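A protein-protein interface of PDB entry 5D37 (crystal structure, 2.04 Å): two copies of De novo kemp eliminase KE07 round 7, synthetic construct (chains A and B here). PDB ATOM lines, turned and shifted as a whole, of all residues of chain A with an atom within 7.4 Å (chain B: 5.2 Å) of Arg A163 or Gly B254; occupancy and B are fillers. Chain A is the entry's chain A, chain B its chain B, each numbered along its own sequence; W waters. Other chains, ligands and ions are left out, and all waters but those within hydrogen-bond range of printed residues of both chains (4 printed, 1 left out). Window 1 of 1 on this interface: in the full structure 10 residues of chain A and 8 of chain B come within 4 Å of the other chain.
NH2 of Arg A163 lies within hydrogen-bond range of O of Glu B251. The side-chain hydroxyl of Ser A122 lies within hydrogen-bond range of a ring nitrogen (NE2) of His B259 (3.2 Å). The guanidinium group (NH1) of Arg A163 lies within hydrogen-bond range of the backbone carbonyl oxygen (O) of Leu B253. NH1 of Arg A163 sits close to O of Gly B254, at 3.3 Å. OG of Ser B255 lies within hydrogen-bond range of NH2 of Arg A163, at 3.3 Å. OG of Ser A111 lies within hydrogen-bond range of O of Leu B253.
The side-chain carboxylate of Glu A159 is in salt-bridge range of the guanidinium group of Arg A163 (2.9 Å). The backbone carbonyl oxygen of Arg A163 lies within hydrogen-bond range of the side-chain hydroxyl of Thr A114 (3.0 Å). OG of Ser A122 lies within hydrogen-bond range of O of Gly A164, at 3.0 Å. The backbone carbonyl oxygen (O) of Ser A122 sits close to the backbone NH (N) of Gly A166, 3.3 Å away. O of Gly B252 is in hydrogen-bond range of OG of Ser B255 (3.0 Å). The side-chain hydroxyl (OG) of Ser A111 lies within hydrogen-bond range of the guanidinium group (NH1) of Arg A163 (3.2 Å).
Among the printed residues, pairs that only touch across the chains: Pro A110 with Glu B251, Ser A111 with Gly B254, Thr A114 with His B259, Ala A117 with His B259, Gln A118 with His B259 and Gly A164 with His B259.
Printed residues of chain B within 4 Å of Arg A163: Glu B251 (3.2 Å), Leu B253 (3.0 Å), Gly B254 (3.3 Å) and Ser B255 (3.3 Å). Printed residues of chain A within 4 Å of Gly B254: Ser A111 and Arg A163. Of the printed residues of chain B, Ser A111 touches Leu B253 and Gly B254. Printed residues of chain B within 4 Å of Thr A114: His B259. Of the printed residues of chain B, Pro A110 touches Glu B251. Of the printed residues of chain B, Ser A122 touches His B259. The nearest printed residue of chain B that does not touch Arg A163 is His B259 (4.01 Å). The nearest residue of chain A that does not touch Gly B254 is Thr A114 (5.5 Å). The nearest printed residue of chain A that does not touch His B259 is Arg A163 (4.01 Å).
Hydrophobic or aromatic side chains of chain A that line the printed part of chain B: Pro A110 and Ala A117. Among the printed residues, 12 pairs touch across the chains. Among the printed residues, no Asp or Glu carboxylate lies within 4 Å of a Lys or Arg side-chain nitrogen of the other chain.
No position is printed for both chains.
Water W1 lies within hydrogen-bond range of the backbone carbonyl oxygen (O) of Lys A162 (2.7 Å), a ring nitrogen (ND1) of His B259 (2.8 Å) and the backbone carbonyl oxygen (O) of Arg A163 (3.5 Å). Water W2 lies within hydrogen-bond range of the guanidinium group of Arg A163, the backbone carbonyl oxygen of Gly B254 and the side-chain hydroxyl of Thr A114. Water W4 bridges OE2 of Glu A159 and OG of Ser B255. Water W3 bridges OG of Ser A111 (3.1 Å) and NH2 of Arg B235 (3.3 Å).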
ATOM      1  N   ALA A 106     -16.814  15.627  -7.413  1.00  0.00           N
ATOM      2  CA  ALA A 106     -18.197  15.976  -7.086  1.00  0.00           C
ATOM      3  C   ALA A 106     -19.099  15.737  -8.294  1.00  0.00           C
ATOM      4  O   ALA A 106     -20.188  15.165  -8.172  1.00  0.00           O
ATOM      5  CB  ALA A 106     -18.295  17.426  -6.641  1.00  0.00           C
ATOM      6  N   ASN A 109     -19.235  11.909  -8.895  1.00  0.00           N
ATOM      7  CA  ASN A 109     -19.871  11.229  -7.772  1.00  0.00           C
ATOM      8  C   ASN A 109     -20.405  12.230  -6.738  1.00  0.00           C
ATOM      9  O   ASN A 109     -19.721  12.544  -5.769  1.00  0.00           O
ATOM     10  CB  ASN A 109     -18.883  10.259  -7.124  1.00  0.00           C
ATOM     11  CG  ASN A 109     -19.456   9.569  -5.903  1.00  0.00           C
ATOM     12  OD1 ASN A 109     -20.657   9.316  -5.828  1.00  0.00           O
ATOM     13  ND2 ASN A 109     -18.593   9.282  -4.924  1.00  0.00           N
ATOM     14  N   PRO A 110     -21.641  12.722  -6.941  1.00  0.00           N
ATOM     15  CA  PRO A 110     -22.210  13.798  -6.103  1.00  0.00           C
ATOM     16  C   PRO A 110     -22.534  13.365  -4.687  1.00  0.00           C
ATOM     17  O   PRO A 110     -22.771  14.248  -3.852  1.00  0.00           O
ATOM     18  CB  PRO A 110     -23.495  14.190  -6.838  1.00  0.00           C
ATOM     19  CG  PRO A 110     -23.354  13.619  -8.247  1.00  0.00           C
ATOM     20  CD  PRO A 110     -22.515  12.376  -8.078  1.00  0.00           C
ATOM     21  N   SER A 111     -22.565  12.051  -4.426  1.00  0.00           N
ATOM     22  CA  SER A 111     -22.701  11.539  -3.063  1.00  0.00           C
ATOM     23  C   SER A 111     -21.537  12.041  -2.209  1.00  0.00           C
ATOM     24  O   SER A 111     -21.662  12.157  -0.989  1.00  0.00           O
ATOM     25  CB  SER A 111     -22.747   9.998  -3.034  1.00  0.00           C
ATOM     26  OG  SER A 111     -23.902   9.486  -3.681  1.00  0.00           O
ATOM     27  N   LEU A 112     -20.414  12.351  -2.857  1.00  0.00           N
ATOM     28  CA  LEU A 112     -19.207  12.802  -2.147  1.00  0.00           C
ATOM     29  C   LEU A 112     -19.483  14.075  -1.371  1.00  0.00           C
ATOM     30  O   LEU A 112     -19.019  14.225  -0.251  1.00  0.00           O
ATOM     31  CB  LEU A 112     -18.038  13.021  -3.111  1.00  0.00           C
ATOM     32  CG  LEU A 112     -16.837  13.774  -2.525  1.00  0.00           C
ATOM     33  CD1 LEU A 112     -16.218  12.990  -1.375  1.00  0.00           C
ATOM     34  CD2 LEU A 112     -15.811  14.062  -3.598  1.00  0.00           C
ATOM     35  N   ILE A 113     -20.275  14.970  -1.961  1.00  0.00           N
ATOM     36  CA  ILE A 113     -20.787  16.142  -1.252  1.00  0.00           C
ATOM     37  C   ILE A 113     -21.486  15.747   0.047  1.00  0.00           C
ATOM     38  O   ILE A 113     -21.134  16.225   1.128  1.00  0.00           O
ATOM     39  CB  ILE A 113     -21.789  16.946  -2.121  1.00  0.00           C
ATOM     40  CG1 ILE A 113     -21.120  17.412  -3.409  1.00  0.00           C
ATOM     41  CG2 ILE A 113     -22.308  18.150  -1.378  1.00  0.00           C
ATOM     42  CD1 ILE A 113     -22.079  17.999  -4.398  1.00  0.00           C
ATOM     43  N   THR A 114     -22.482  14.879  -0.065  1.00  0.00           N
ATOM     44  CA  THR A 114     -23.284  14.508   1.091  1.00  0.00           C
ATOM     45  C   THR A 114     -22.417  13.838   2.161  1.00  0.00           C
ATOM     46  O   THR A 114     -22.542  14.149   3.338  1.00  0.00           O
ATOM     47  CB  THR A 114     -24.432  13.588   0.668  1.00  0.00           C
ATOM     48  OG1 THR A 114     -24.914  14.024  -0.605  1.00  0.00           O
ATOM     49  CG2 THR A 114     -25.583  13.615   1.685  1.00  0.00           C
ATOM     50  N   GLN A 115     -21.520  12.950   1.741  1.00  0.00           N
ATOM     51  CA  GLN A 115     -20.637  12.240   2.665  1.00  0.00           C
ATOM     52  C   GLN A 115     -19.894  13.184   3.581  1.00  0.00           C
ATOM     53  O   GLN A 115     -19.997  13.075   4.794  1.00  0.00           O
ATOM     54  CB  GLN A 115     -19.637  11.382   1.902  1.00  0.00           C
ATOM     55  CG  GLN A 115     -20.282  10.216   1.199  1.00  0.00           C
ATOM     56  CD  GLN A 115     -19.328   9.502   0.279  1.00  0.00           C
ATOM     57  OE1 GLN A 115     -18.107   9.682   0.365  1.00  0.00           O
ATOM     58  NE2 GLN A 115     -19.874   8.692  -0.622  1.00  0.00           N
ATOM     59  N   ALA A 117     -20.485  16.450   4.080  1.00  0.00           N
ATOM     60  CA  ALA A 117     -21.491  17.250   4.810  1.00  0.00           C
ATOM     61  C   ALA A 117     -22.129  16.522   6.031  1.00  0.00           C
ATOM     62  O   ALA A 117     -22.312  17.126   7.097  1.00  0.00           O
ATOM     63  CB  ALA A 117     -22.578  17.699   3.847  1.00  0.00           C
ATOM     64  N   GLN A 118     -22.451  15.239   5.862  1.00  0.00           N
ATOM     65  CA  GLN A 118     -23.037  14.383   6.899  1.00  0.00           C
ATOM     66  C   GLN A 118     -22.219  14.383   8.185  1.00  0.00           C
ATOM     67  O   GLN A 118     -22.751  14.266   9.297  1.00  0.00           O
ATOM     68  CB  GLN A 118     -23.158  12.930   6.403  1.00  0.00           C
ATOM     69  CG  GLN A 118     -24.211  12.666   5.355  1.00  0.00           C
ATOM     70  CD  GLN A 118     -24.325  11.188   4.967  1.00  0.00           C
ATOM     71  OE1 GLN A 118     -23.452  10.633   4.297  1.00  0.00           O
ATOM     72  NE2 GLN A 118     -25.420  10.556   5.375  1.00  0.00           N
ATOM     73  N   SER A 122     -22.682  21.138   6.230  1.00  0.00           N
ATOM     74  CA  SER A 122     -22.618  21.809   4.920  1.00  0.00           C
ATOM     75  C   SER A 122     -21.568  22.899   4.890  1.00  0.00           C
ATOM     76  O   SER A 122     -20.909  23.093   3.872  1.00  0.00           O
ATOM     77  CB  SER A 122     -23.962  22.426   4.548  1.00  0.00           C
ATOM     78  OG  SER A 122     -24.963  21.441   4.443  1.00  0.00           O
ATOM     79  N   VAL A 125     -18.246  22.428   3.213  1.00  0.00           N
ATOM     80  CA  VAL A 125     -18.194  21.960   1.830  1.00  0.00           C
ATOM     81  C   VAL A 125     -18.326  23.065   0.775  1.00  0.00           C
ATOM     82  O   VAL A 125     -19.385  23.723   0.624  1.00  0.00           O
ATOM     83  CB  VAL A 125     -19.300  20.905   1.552  1.00  0.00           C
ATOM     84  CG1 VAL A 125     -19.097  20.289   0.178  1.00  0.00           C
ATOM     85  CG2 VAL A 125     -19.299  19.826   2.626  1.00  0.00           C
ATOM     86  N   TRP A 156     -26.757  21.424 -12.575  1.00  0.00           N
ATOM     87  CA  TRP A 156     -25.716  21.097 -11.600  1.00  0.00           C
ATOM     88  C   TRP A 156     -25.895  21.919 -10.331  1.00  0.00           C
ATOM     89  O   TRP A 156     -25.819  21.383  -9.230  1.00  0.00           O
ATOM     90  CB  TRP A 156     -24.315  21.299 -12.200  1.00  0.00           C
ATOM     91  CG  TRP A 156     -23.158  20.863 -11.301  1.00  0.00           C
ATOM     92  CD1 TRP A 156     -21.995  21.540 -11.094  1.00  0.00           C
ATOM     93  CD2 TRP A 156     -23.092  19.696 -10.471  1.00  0.00           C
ATOM     94  NE1 TRP A 156     -21.197  20.863 -10.198  1.00  0.00           N
ATOM     95  CE2 TRP A 156     -21.847  19.724  -9.809  1.00  0.00           C
ATOM     96  CE3 TRP A 156     -23.954  18.620 -10.239  1.00  0.00           C
ATOM     97  CZ2 TRP A 156     -21.452  18.725  -8.933  1.00  0.00           C
ATOM     98  CZ3 TRP A 156     -23.558  17.629  -9.372  1.00  0.00           C
ATOM     99  CH2 TRP A 156     -22.324  17.688  -8.723  1.00  0.00           C
ATOM    100  N   VAL A 157     -26.162  23.212 -10.483  1.00  0.00           N
ATOM    101  CA  VAL A 157     -26.375  24.084  -9.320  1.00  0.00           C
ATOM    102  C   VAL A 157     -27.456  23.589  -8.332  1.00  0.00           C
ATOM    103  O   VAL A 157     -27.256  23.600  -7.111  1.00  0.00           O
ATOM    104  CB  VAL A 157     -26.721  25.505  -9.782  1.00  0.00           C
ATOM    105  CG1 VAL A 157     -27.372  26.298  -8.672  1.00  0.00           C
ATOM    106  CG2 VAL A 157     -25.449  26.195 -10.290  1.00  0.00           C
ATOM    107  N   VAL A 158     -28.579  23.120  -8.860  1.00  0.00           N
ATOM    108  CA  VAL A 158     -29.676  22.648  -8.024  1.00  0.00           C
ATOM    109  C   VAL A 158     -29.302  21.322  -7.351  1.00  0.00           C
ATOM    110  O   VAL A 158     -29.508  21.136  -6.160  1.00  0.00           O
ATOM    111  CB  VAL A 158     -30.959  22.477  -8.846  1.00  0.00           C
ATOM    112  CG1 VAL A 158     -32.059  21.842  -8.004  1.00  0.00           C
ATOM    113  CG2 VAL A 158     -31.407  23.820  -9.405  1.00  0.00           C
ATOM    114  N   GLU A 159     -28.729  20.413  -8.130  1.00  0.00           N
ATOM    115  CA  GLU A 159     -28.184  19.174  -7.589  1.00  0.00           C
ATOM    116  C   GLU A 159     -27.135  19.478  -6.494  1.00  0.00           C
ATOM    117  O   GLU A 159     -27.081  18.792  -5.477  1.00  0.00           O
ATOM    118  CB  GLU A 159     -27.587  18.332  -8.723  1.00  0.00           C
ATOM    119  CG  GLU A 159     -27.238  16.860  -8.375  1.00  0.00           C
ATOM    120  CD  GLU A 159     -28.438  16.024  -7.917  1.00  0.00           C
ATOM    121  OE1 GLU A 159     -28.297  15.253  -6.942  1.00  0.00           O
ATOM    122  OE2 GLU A 159     -29.522  16.131  -8.517  1.00  0.00           O
ATOM    123  N   VAL A 160     -26.317  20.509  -6.689  1.00  0.00           N
ATOM    124  CA  VAL A 160     -25.246  20.786  -5.719  1.00  0.00           C
ATOM    125  C   VAL A 160     -25.848  21.198  -4.358  1.00  0.00           C
ATOM    126  O   VAL A 160     -25.448  20.678  -3.319  1.00  0.00           O
ATOM    127  CB  VAL A 160     -24.262  21.861  -6.242  1.00  0.00           C
ATOM    128  CG1 VAL A 160     -23.469  22.499  -5.108  1.00  0.00           C
ATOM    129  CG2 VAL A 160     -23.306  21.255  -7.245  1.00  0.00           C
ATOM    130  N   GLU A 161     -26.822  22.101  -4.360  1.00  0.00           N
ATOM    131  CA  GLU A 161     -27.489  22.464  -3.102  1.00  0.00           C
ATOM    132  C   GLU A 161     -28.275  21.292  -2.510  1.00  0.00           C
ATOM    133  O   GLU A 161     -28.298  21.108  -1.299  1.00  0.00           O
ATOM    134  CB  GLU A 161     -28.422  23.659  -3.294  1.00  0.00           C
ATOM    135  CG  GLU A 161     -29.013  24.194  -1.985  1.00  0.00           C
ATOM    136  CD  GLU A 161     -29.981  25.352  -2.212  1.00  0.00           C
ATOM    137  OE1 GLU A 161     -29.878  26.012  -3.254  1.00  0.00           O
ATOM    138  OE2 GLU A 161     -30.849  25.595  -1.357  1.00  0.00           O
ATOM    139  N   LYS A 162     -28.918  20.505  -3.366  1.00  0.00           N
ATOM    140  CA  LYS A 162     -29.709  19.375  -2.889  1.00  0.00           C
ATOM    141  C   LYS A 162     -28.827  18.365  -2.127  1.00  0.00           C
ATOM    142  O   LYS A 162     -29.242  17.811  -1.107  1.00  0.00           O
ATOM    143  CB  LYS A 162     -30.441  18.712  -4.070  1.00  0.00           C
ATOM    144  CG  LYS A 162     -31.240  17.467  -3.725  1.00  0.00           C
ATOM    145  CD  LYS A 162     -31.786  16.798  -4.993  1.00  0.00           C
ATOM    146  CE  LYS A 162     -32.497  15.487  -4.677  1.00  0.00           C
ATOM    147  NZ  LYS A 162     -32.883  14.737  -5.924  1.00  0.00           N
ATOM    148  N   ARG A 163     -27.602  18.147  -2.595  1.00  0.00           N
ATOM    149  CA  ARG A 163     -26.723  17.159  -1.953  1.00  0.00           C
ATOM    150  C   ARG A 163     -26.074  17.669  -0.656  1.00  0.00           C
ATOM    151  O   ARG A 163     -25.407  16.902   0.056  1.00  0.00           O
ATOM    152  CB  ARG A 163     -25.625  16.713  -2.929  1.00  0.00           C
ATOM    153  CG  ARG A 163     -26.134  15.997  -4.181  1.00  0.00           C
ATOM    154  CD  ARG A 163     -26.079  14.471  -4.034  1.00  0.00           C
ATOM    155  NE  ARG A 163     -26.482  13.772  -5.262  1.00  0.00           N
ATOM    156  CZ  ARG A 163     -26.488  12.453  -5.397  1.00  0.00           C
ATOM    157  NH1 ARG A 163     -26.123  11.686  -4.377  1.00  0.00           N
ATOM    158  NH2 ARG A 163     -26.876  11.902  -6.539  1.00  0.00           N
ATOM    159  N   GLY A 164     -26.263  18.952  -0.350  1.00  0.00           N
ATOM    160  CA  GLY A 164     -25.786  19.529   0.904  1.00  0.00           C
ATOM    161  C   GLY A 164     -24.475  20.306   0.889  1.00  0.00           C
ATOM    162  O   GLY A 164     -23.778  20.389   1.907  1.00  0.00           O
ATOM    163  N   ALA A 165     -24.137  20.899  -0.252  1.00  0.00           N
ATOM    164  CA  ALA A 165     -22.963  21.740  -0.335  1.00  0.00           C
ATOM    165  C   ALA A 165     -23.241  23.081   0.372  1.00  0.00           C
ATOM    166  O   ALA A 165     -24.384  23.533   0.438  1.00  0.00           O
ATOM    167  CB  ALA A 165     -22.556  21.962  -1.784  1.00  0.00           C
ATOM    168  N   GLY A 166     -22.185  23.704   0.888  1.00  0.00           N
ATOM    169  CA  GLY A 166     -22.298  24.921   1.674  1.00  0.00           C
ATOM    170  C   GLY A 166     -22.159  26.249   0.941  1.00  0.00           C
ATOM    171  O   GLY A 166     -22.746  27.246   1.377  1.00  0.00           O
ATOM    172  N   GLU B  41     -33.243   6.000  -8.926  1.00  0.00           N
ATOM    173  CA  GLU B  41     -32.714   6.831  -7.846  1.00  0.00           C
ATOM    174  C   GLU B  41     -31.573   6.210  -7.043  1.00  0.00           C
ATOM    175  O   GLU B  41     -31.032   6.848  -6.137  1.00  0.00           O
ATOM    176  CB  GLU B  41     -33.850   7.195  -6.902  1.00  0.00           C
ATOM    177  CG  GLU B  41     -35.025   7.812  -7.614  1.00  0.00           C
ATOM    178  CD  GLU B  41     -36.224   7.980  -6.710  1.00  0.00           C
ATOM    179  OE1 GLU B  41     -36.740   6.955  -6.199  1.00  0.00           O
ATOM    180  OE2 GLU B  41     -36.640   9.136  -6.501  1.00  0.00           O
ATOM    181  N   ILE B  42     -31.201   4.968  -7.360  1.00  0.00           N
ATOM    182  CA  ILE B  42     -30.172   4.291  -6.574  1.00  0.00           C
ATOM    183  C   ILE B  42     -29.024   3.725  -7.403  1.00  0.00           C
ATOM    184  O   ILE B  42     -28.177   3.026  -6.871  1.00  0.00           O
ATOM    185  CB  ILE B  42     -30.770   3.127  -5.737  1.00  0.00           C
ATOM    186  CG1 ILE B  42     -31.157   1.946  -6.628  1.00  0.00           C
ATOM    187  CG2 ILE B  42     -31.970   3.593  -4.900  1.00  0.00           C
ATOM    188  CD1 ILE B  42     -31.898   0.857  -5.870  1.00  0.00           C
ATOM    189  N   ARG B 235     -25.999  -0.401  -5.863  1.00  0.00           N
ATOM    190  CA  ARG B 235     -24.944   0.453  -5.371  1.00  0.00           C
ATOM    191  C   ARG B 235     -23.647  -0.336  -5.206  1.00  0.00           C
ATOM    192  O   ARG B 235     -22.629   0.040  -5.774  1.00  0.00           O
ATOM    193  CB  ARG B 235     -25.359   1.101  -4.041  1.00  0.00           C
ATOM    194  CG  ARG B 235     -24.217   1.680  -3.276  1.00  0.00           C
ATOM    195  CD  ARG B 235     -24.664   2.071  -1.881  1.00  0.00           C
ATOM    196  NE  ARG B 235     -24.717   3.517  -1.736  1.00  0.00           N
ATOM    197  CZ  ARG B 235     -25.366   4.153  -0.766  1.00  0.00           C
ATOM    198  NH1 ARG B 235     -26.042   3.468   0.153  1.00  0.00           N
ATOM    199  NH2 ARG B 235     -25.349   5.480  -0.728  1.00  0.00           N
ATOM    200  N   GLU B 251     -23.449   8.650 -10.901  1.00  0.00           N
ATOM    201  CA  GLU B 251     -24.177   9.866 -10.628  1.00  0.00           C
ATOM    202  C   GLU B 251     -25.532   9.605  -9.983  1.00  0.00           C
ATOM    203  O   GLU B 251     -26.102  10.489  -9.359  1.00  0.00           O
ATOM    204  CB  GLU B 251     -24.326  10.672 -11.923  1.00  0.00           C
ATOM    205  CG  GLU B 251     -23.015  11.276 -12.402  1.00  0.00           C
ATOM    206  CD  GLU B 251     -22.360  10.496 -13.532  1.00  0.00           C
ATOM    207  OE1 GLU B 251     -22.749   9.332 -13.777  1.00  0.00           O
ATOM    208  OE2 GLU B 251     -21.453  11.061 -14.182  1.00  0.00           O
ATOM    209  N   GLY B 252     -26.031   8.383 -10.122  1.00  0.00           N
ATOM    210  CA  GLY B 252     -27.337   8.022  -9.590  1.00  0.00           C
ATOM    211  C   GLY B 252     -27.230   7.545  -8.156  1.00  0.00           C
ATOM    212  O   GLY B 252     -28.215   7.540  -7.409  1.00  0.00           O
ATOM    213  N   LEU B 253     -26.026   7.135  -7.768  1.00  0.00           N
ATOM    214  CA  LEU B 253     -25.807   6.676  -6.411  1.00  0.00           C
ATOM    215  C   LEU B 253     -26.217   7.763  -5.430  1.00  0.00           C
ATOM    216  O   LEU B 253     -25.943   8.948  -5.642  1.00  0.00           O
ATOM    217  CB  LEU B 253     -24.347   6.286  -6.186  1.00  0.00           C
ATOM    218  CG  LEU B 253     -23.755   5.276  -7.172  1.00  0.00           C
ATOM    219  CD1 LEU B 253     -22.447   4.721  -6.636  1.00  0.00           C
ATOM    220  CD2 LEU B 253     -24.731   4.154  -7.452  1.00  0.00           C
ATOM    221  N   GLY B 254     -26.915   7.340  -4.380  1.00  0.00           N
ATOM    222  CA  GLY B 254     -27.136   8.164  -3.215  1.00  0.00           C
ATOM    223  C   GLY B 254     -28.157   9.260  -3.369  1.00  0.00           C
ATOM    224  O   GLY B 254     -28.314  10.073  -2.461  1.00  0.00           O
ATOM    225  N   SER B 255     -28.862   9.279  -4.500  1.00  0.00           N
ATOM    226  CA  SER B 255     -29.817  10.350  -4.799  1.00  0.00           C
ATOM    227  C   SER B 255     -30.879  10.552  -3.734  1.00  0.00           C
ATOM    228  O   SER B 255     -31.394  11.653  -3.570  1.00  0.00           O
ATOM    229  CB  SER B 255     -30.528  10.091  -6.133  1.00  0.00           C
ATOM    230  OG  SER B 255     -29.632  10.171  -7.224  1.00  0.00           O
ATOM    231  N   LEU B 256     -31.221   9.487  -3.021  1.00  0.00           N
ATOM    232  CA  LEU B 256     -32.333   9.548  -2.095  1.00  0.00           C
ATOM    233  C   LEU B 256     -31.848   9.891  -0.711  1.00  0.00           C
ATOM    234  O   LEU B 256     -32.626   9.882   0.246  1.00  0.00           O
ATOM    235  CB  LEU B 256     -33.095   8.225  -2.070  1.00  0.00           C
ATOM    236  CG  LEU B 256     -33.778   7.848  -3.385  1.00  0.00           C
ATOM    237  CD1 LEU B 256     -34.601   6.599  -3.208  1.00  0.00           C
ATOM    238  CD2 LEU B 256     -34.639   9.003  -3.878  1.00  0.00           C
ATOM    239  N   GLU B 257     -30.558  10.191  -0.601  1.00  0.00           N
ATOM    240  CA  GLU B 257     -29.943  10.317   0.706  1.00  0.00           C
ATOM    241  C   GLU B 257     -29.585  11.775   0.983  1.00  0.00           C
ATOM    242  O   GLU B 257     -29.411  12.561   0.052  1.00  0.00           O
ATOM    243  CB  GLU B 257     -28.705   9.409   0.803  1.00  0.00           C
ATOM    244  CG  GLU B 257     -28.962   7.943   0.400  1.00  0.00           C
ATOM    245  CD  GLU B 257     -27.725   7.060   0.529  1.00  0.00           C
ATOM    246  OE1 GLU B 257     -26.591   7.587   0.436  1.00  0.00           O
ATOM    247  OE2 GLU B 257     -27.888   5.836   0.727  1.00  0.00           O
ATOM    248  N   HIS B 259     -27.938  14.913   4.161  1.00  0.00           N
ATOM    249  CA  HIS B 259     -26.848  15.176   5.112  1.00  0.00           C
ATOM    250  C   HIS B 259     -27.379  15.509   6.496  1.00  0.00           C
ATOM    251  O   HIS B 259     -26.715  16.194   7.276  1.00  0.00           O
ATOM    252  CB  HIS B 259     -25.951  16.321   4.619  1.00  0.00           C
ATOM    253  CG  HIS B 259     -26.692  17.595   4.351  1.00  0.00           C
ATOM    254  ND1 HIS B 259     -27.596  17.724   3.316  1.00  0.00           N
ATOM    255  CD2 HIS B 259     -26.658  18.797   4.976  1.00  0.00           C
ATOM    256  CE1 HIS B 259     -28.091  18.948   3.318  1.00  0.00           C
ATOM    257  NE2 HIS B 259     -27.538  19.619   4.317  1.00  0.00           N
HETATM  258  O   HOH W   1     -28.690  16.312   1.103  1.00  0.00           O
HETATM  259  O   HOH W   2     -26.288  11.767  -1.628  1.00  0.00           O
HETATM  260  O   HOH W   3     -23.119   6.540  -2.973  1.00  0.00           O
HETATM  261  O   HOH W   4     -29.674  13.071  -8.697  1.00  0.00           O
